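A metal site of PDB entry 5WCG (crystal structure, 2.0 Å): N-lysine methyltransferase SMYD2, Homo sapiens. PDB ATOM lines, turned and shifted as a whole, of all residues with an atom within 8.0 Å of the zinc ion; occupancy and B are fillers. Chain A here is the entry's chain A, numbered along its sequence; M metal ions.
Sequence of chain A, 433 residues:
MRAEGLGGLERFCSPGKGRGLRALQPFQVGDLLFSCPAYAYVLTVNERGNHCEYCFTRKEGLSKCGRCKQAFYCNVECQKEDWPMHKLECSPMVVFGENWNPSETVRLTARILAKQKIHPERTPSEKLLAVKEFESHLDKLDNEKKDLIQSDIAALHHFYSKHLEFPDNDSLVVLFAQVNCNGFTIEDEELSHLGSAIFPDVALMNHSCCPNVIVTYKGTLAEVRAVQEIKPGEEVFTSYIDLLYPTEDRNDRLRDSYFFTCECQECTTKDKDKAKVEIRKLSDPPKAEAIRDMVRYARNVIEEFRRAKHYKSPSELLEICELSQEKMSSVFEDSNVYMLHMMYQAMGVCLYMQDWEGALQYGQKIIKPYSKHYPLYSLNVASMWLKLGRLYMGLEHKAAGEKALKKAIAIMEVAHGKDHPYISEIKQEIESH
SG of Cys 78 binds the zinc ion.
The side-chain sulfur (SG) of Cys 52 binds the zinc ion.
SG of Cys 55 binds the zinc ion, 2.4 Å away.
The zinc ion is bound by SG of Cys 74.
The side-chain sulfur (SG) of Cys 52 sits close to the backbone NH (N) of Tyr 54, at 3.4 Å.
OD1 of Asn 75 lies within hydrogen-bond range of N of Cys 78 (3.0 Å).
The backbone carbonyl oxygen (O) of Thr 57 lies within hydrogen-bond range of the backbone NH (N) of Cys 52, at 2.9 Å.
The side-chain sulfur (SG) of Cys 55 lies close to the side-chain hydroxyl (OG1) of Thr 57 (3.0 Å).
The nearest printed residue that does not touch the zinc ion is Thr 57 (4.6 Å).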
ATOM      1  N   HIS A  51      22.609 -11.327  12.049  1.00  0.00           N
ATOM      2  CA  HIS A  51      23.460 -10.475  12.897  1.00  0.00           C
ATOM      3  C   HIS A  51      22.767 -10.209  14.225  1.00  0.00           C
ATOM      4  O   HIS A  51      21.539 -10.122  14.283  1.00  0.00           O
ATOM      5  CB  HIS A  51      23.736  -9.132  12.203  1.00  0.00           C
ATOM      6  CG  HIS A  51      24.504  -9.245  10.925  1.00  0.00           C
ATOM      7  ND1 HIS A  51      25.849  -8.941  10.831  1.00  0.00           N
ATOM      8  CD2 HIS A  51      24.114  -9.614   9.682  1.00  0.00           C
ATOM      9  CE1 HIS A  51      26.246  -9.147   9.587  1.00  0.00           C
ATOM     10  NE2 HIS A  51      25.219  -9.548   8.874  1.00  0.00           N
ATOM     11  N   CYS A  52      23.560 -10.075  15.286  1.00  0.00           N
ATOM     12  CA  CYS A  52      23.048  -9.601  16.574  1.00  0.00           C
ATOM     13  C   CYS A  52      22.576  -8.143  16.447  1.00  0.00           C
ATOM     14  O   CYS A  52      23.298  -7.315  15.893  1.00  0.00           O
ATOM     15  CB  CYS A  52      24.114  -9.720  17.636  1.00  0.00           C
ATOM     16  SG  CYS A  52      23.649  -9.043  19.258  1.00  0.00           S
ATOM     17  N   GLU A  53      21.372  -7.838  16.936  1.00  0.00           N
ATOM     18  CA  GLU A  53      20.814  -6.479  16.819  1.00  0.00           C
ATOM     19  C   GLU A  53      21.631  -5.500  17.639  1.00  0.00           C
ATOM     20  O   GLU A  53      21.671  -4.311  17.312  1.00  0.00           O
ATOM     21  CB  GLU A  53      19.390  -6.390  17.379  1.00  0.00           C
ATOM     22  CG  GLU A  53      18.345  -7.243  16.687  1.00  0.00           C
ATOM     23  CD  GLU A  53      17.555  -6.527  15.605  1.00  0.00           C
ATOM     24  OE1 GLU A  53      17.237  -7.203  14.637  1.00  0.00           O
ATOM     25  OE2 GLU A  53      17.207  -5.326  15.751  1.00  0.00           O
ATOM     26  N   TYR A  54      22.223  -5.955  18.735  1.00  0.00           N
ATOM     27  CA  TYR A  54      22.949  -5.047  19.612  1.00  0.00           C
ATOM     28  C   TYR A  54      24.356  -4.761  19.120  1.00  0.00           C
ATOM     29  O   TYR A  54      24.765  -3.605  19.078  1.00  0.00           O
ATOM     30  CB  TYR A  54      23.016  -5.580  21.039  1.00  0.00           C
ATOM     31  CG  TYR A  54      23.732  -4.625  21.989  1.00  0.00           C
ATOM     32  CD1 TYR A  54      23.166  -3.405  22.343  1.00  0.00           C
ATOM     33  CD2 TYR A  54      24.986  -4.942  22.488  1.00  0.00           C
ATOM     34  CE1 TYR A  54      23.829  -2.540  23.195  1.00  0.00           C
ATOM     35  CE2 TYR A  54      25.661  -4.096  23.337  1.00  0.00           C
ATOM     36  CZ  TYR A  54      25.074  -2.900  23.688  1.00  0.00           C
ATOM     37  OH  TYR A  54      25.764  -2.089  24.517  1.00  0.00           O
ATOM     38  N   CYS A  55      25.111  -5.796  18.809  1.00  0.00           N
ATOM     39  CA  CYS A  55      26.534  -5.610  18.497  1.00  0.00           C
ATOM     40  C   CYS A  55      26.907  -5.888  17.041  1.00  0.00           C
ATOM     41  O   CYS A  55      28.062  -5.720  16.697  1.00  0.00           O
ATOM     42  CB  CYS A  55      27.382  -6.499  19.429  1.00  0.00           C
ATOM     43  SG  CYS A  55      27.322  -8.251  19.049  1.00  0.00           S
ATOM     44  N   PHE A  56      25.966  -6.325  16.216  1.00  0.00           N
ATOM     45  CA  PHE A  56      26.173  -6.639  14.793  1.00  0.00           C
ATOM     46  C   PHE A  56      27.107  -7.832  14.483  1.00  0.00           C
ATOM     47  O   PHE A  56      27.469  -8.012  13.318  1.00  0.00           O
ATOM     48  CB  PHE A  56      26.621  -5.395  13.987  1.00  0.00           C
ATOM     49  CG  PHE A  56      25.528  -4.416  13.629  1.00  0.00           C
ATOM     50  CD1 PHE A  56      24.446  -4.150  14.497  1.00  0.00           C
ATOM     51  CD2 PHE A  56      25.612  -3.683  12.456  1.00  0.00           C
ATOM     52  CE1 PHE A  56      23.463  -3.234  14.139  1.00  0.00           C
ATOM     53  CE2 PHE A  56      24.617  -2.748  12.100  1.00  0.00           C
ATOM     54  CZ  PHE A  56      23.553  -2.526  12.952  1.00  0.00           C
ATOM     55  N   THR A  57      27.473  -8.643  15.481  1.00  0.00           N
ATOM     56  CA  THR A  57      28.215  -9.883  15.240  1.00  0.00           C
ATOM     57  C   THR A  57      27.411 -10.780  14.310  1.00  0.00           C
ATOM     58  O   THR A  57      26.215 -10.991  14.539  1.00  0.00           O
ATOM     59  CB  THR A  57      28.515 -10.622  16.568  1.00  0.00           C
ATOM     60  OG1 THR A  57      29.316  -9.778  17.399  1.00  0.00           O
ATOM     61  CG2 THR A  57      29.265 -11.938  16.335  1.00  0.00           C
ATOM     62  N   ARG A  58      28.065 -11.225  13.243  1.00  0.00           N
ATOM     63  CA  ARG A  58      27.492 -12.128  12.270  1.00  0.00           C
ATOM     64  C   ARG A  58      27.875 -13.575  12.633  1.00  0.00           C
ATOM     65  O   ARG A  58      29.051 -13.948  12.518  1.00  0.00           O
ATOM     66  CB  ARG A  58      28.027 -11.827  10.864  1.00  0.00           C
ATOM     67  CG  ARG A  58      27.383 -12.662   9.764  1.00  0.00           C
ATOM     68  CD  ARG A  58      27.824 -12.244   8.354  1.00  0.00           C
ATOM     69  NE  ARG A  58      29.272 -12.430   8.181  1.00  0.00           N
ATOM     70  CZ  ARG A  58      30.049 -11.781   7.315  1.00  0.00           C
ATOM     71  NH1 ARG A  58      29.552 -10.863   6.486  1.00  0.00           N
ATOM     72  NH2 ARG A  58      31.352 -12.013   7.305  1.00  0.00           N
ATOM     73  N   LYS A  59      26.906 -14.378  13.057  1.00  0.00           N
ATOM     74  CA  LYS A  59      27.152 -15.765  13.444  1.00  0.00           C
ATOM     75  C   LYS A  59      25.871 -16.570  13.394  1.00  0.00           C
ATOM     76  O   LYS A  59      24.781 -16.007  13.275  1.00  0.00           O
ATOM     77  CB  LYS A  59      27.765 -15.834  14.860  1.00  0.00           C
ATOM     78  CG  LYS A  59      26.869 -15.304  15.971  1.00  0.00           C
ATOM     79  CD  LYS A  59      27.540 -15.173  17.335  1.00  0.00           C
ATOM     80  CE  LYS A  59      27.966 -16.491  17.938  1.00  0.00           C
ATOM     81  NZ  LYS A  59      26.836 -17.456  18.009  1.00  0.00           N
ATOM     82  N   LEU A  62      21.938 -17.520  16.884  1.00  0.00           N
ATOM     83  CA  LEU A  62      21.504 -16.375  17.661  1.00  0.00           C
ATOM     84  C   LEU A  62      20.163 -16.699  18.272  1.00  0.00           C
ATOM     85  O   LEU A  62      19.291 -17.311  17.639  1.00  0.00           O
ATOM     86  CB  LEU A  62      21.377 -15.136  16.773  1.00  0.00           C
ATOM     87  CG  LEU A  62      22.633 -14.585  16.095  1.00  0.00           C
ATOM     88  CD1 LEU A  62      22.268 -13.556  15.042  1.00  0.00           C
ATOM     89  CD2 LEU A  62      23.589 -13.956  17.115  1.00  0.00           C
ATOM     90  N   PHE A  72      17.131 -10.712  17.067  1.00  0.00           N
ATOM     91  CA  PHE A  72      18.077 -11.787  17.433  1.00  0.00           C
ATOM     92  C   PHE A  72      19.339 -11.221  18.047  1.00  0.00           C
ATOM     93  O   PHE A  72      19.755 -10.080  17.718  1.00  0.00           O
ATOM     94  CB  PHE A  72      18.419 -12.619  16.210  1.00  0.00           C
ATOM     95  CG  PHE A  72      17.229 -13.282  15.588  1.00  0.00           C
ATOM     96  CD1 PHE A  72      16.319 -12.537  14.825  1.00  0.00           C
ATOM     97  CD2 PHE A  72      17.013 -14.647  15.755  1.00  0.00           C
ATOM     98  CE1 PHE A  72      15.195 -13.154  14.262  1.00  0.00           C
ATOM     99  CE2 PHE A  72      15.916 -15.260  15.169  1.00  0.00           C
ATOM    100  CZ  PHE A  72      15.011 -14.515  14.429  1.00  0.00           C
ATOM    101  N   TYR A  73      19.947 -12.027  18.928  1.00  0.00           N
ATOM    102  CA  TYR A  73      21.024 -11.609  19.829  1.00  0.00           C
ATOM    103  C   TYR A  73      22.054 -12.722  20.050  1.00  0.00           C
ATOM    104  O   TYR A  73      21.715 -13.903  19.970  1.00  0.00           O
ATOM    105  CB  TYR A  73      20.436 -11.209  21.180  1.00  0.00           C
ATOM    106  CG  TYR A  73      19.477 -10.024  21.080  1.00  0.00           C
ATOM    107  CD1 TYR A  73      19.974  -8.758  20.842  1.00  0.00           C
ATOM    108  CD2 TYR A  73      18.101 -10.191  21.200  1.00  0.00           C
ATOM    109  CE1 TYR A  73      19.121  -7.671  20.747  1.00  0.00           C
ATOM    110  CE2 TYR A  73      17.236  -9.101  21.100  1.00  0.00           C
ATOM    111  CZ  TYR A  73      17.754  -7.833  20.869  1.00  0.00           C
ATOM    112  OH  TYR A  73      16.934  -6.726  20.783  1.00  0.00           O
ATOM    113  N   CYS A  74      23.309 -12.347  20.342  1.00  0.00           N
ATOM    114  CA  CYS A  74      24.352 -13.342  20.695  1.00  0.00           C
ATOM    115  C   CYS A  74      23.966 -14.155  21.935  1.00  0.00           C
ATOM    116  O   CYS A  74      24.194 -15.345  22.004  1.00  0.00           O
ATOM    117  CB  CYS A  74      25.671 -12.644  20.999  1.00  0.00           C
ATOM    118  SG  CYS A  74      26.321 -11.652  19.657  1.00  0.00           S
ATOM    119  N   ASN A  75      23.368 -13.469  22.908  1.00  0.00           N
ATOM    120  CA  ASN A  75      23.069 -14.037  24.207  1.00  0.00           C
ATOM    121  C   ASN A  75      22.183 -13.046  24.967  1.00  0.00           C
ATOM    122  O   ASN A  75      21.879 -11.933  24.473  1.00  0.00           O
ATOM    123  CB  ASN A  75      24.375 -14.250  24.964  1.00  0.00           C
ATOM    124  CG  ASN A  75      25.185 -12.961  25.099  1.00  0.00           C
ATOM    125  OD1 ASN A  75      24.698 -11.946  25.589  1.00  0.00           O
ATOM    126  ND2 ASN A  75      26.445 -13.017  24.688  1.00  0.00           N
ATOM    127  N   GLU A  77      22.869 -11.106  27.486  1.00  0.00           N
ATOM    128  CA  GLU A  77      23.482  -9.795  27.782  1.00  0.00           C
ATOM    129  C   GLU A  77      23.278  -8.795  26.631  1.00  0.00           C
ATOM    130  O   GLU A  77      22.949  -7.627  26.878  1.00  0.00           O
ATOM    131  CB  GLU A  77      24.952  -9.904  28.199  1.00  0.00           C
ATOM    132  CG  GLU A  77      25.121 -10.662  29.525  1.00  0.00           C
ATOM    133  CD  GLU A  77      26.562 -10.880  29.943  1.00  0.00           C
ATOM    134  OE1 GLU A  77      27.476 -10.327  29.290  1.00  0.00           O
ATOM    135  OE2 GLU A  77      26.814 -11.620  30.939  1.00  0.00           O
ATOM    136  N   CYS A  78      23.481  -9.254  25.388  1.00  0.00           N
ATOM    137  CA  CYS A  78      23.237  -8.414  24.213  1.00  0.00           C
ATOM    138  C   CYS A  78      21.757  -8.018  24.146  1.00  0.00           C
ATOM    139  O   CYS A  78      21.428  -6.870  23.863  1.00  0.00           O
ATOM    140  CB  CYS A  78      23.671  -9.121  22.889  1.00  0.00           C
ATOM    141  SG  CYS A  78      25.475  -9.049  22.579  1.00  0.00           S
ATOM    142  N   GLN A  79      20.880  -8.973  24.428  1.00  0.00           N
ATOM    143  CA  GLN A  79      19.451  -8.758  24.407  1.00  0.00           C
ATOM    144  C   GLN A  79      19.022  -7.719  25.424  1.00  0.00           C
ATOM    145  O   GLN A  79      18.250  -6.826  25.095  1.00  0.00           O
ATOM    146  CB  GLN A  79      18.680 -10.068  24.650  1.00  0.00           C
ATOM    147  CG  GLN A  79      17.174  -9.880  24.811  1.00  0.00           C
ATOM    148  CD  GLN A  79      16.391 -11.181  24.939  1.00  0.00           C
ATOM    149  OE1 GLN A  79      15.170 -11.221  24.699  1.00  0.00           O
ATOM    150  NE2 GLN A  79      17.071 -12.235  25.311  1.00  0.00           N
HETATM  151 ZN    ZN M   1      25.722  -9.448  20.286  1.00  0.00          ZN
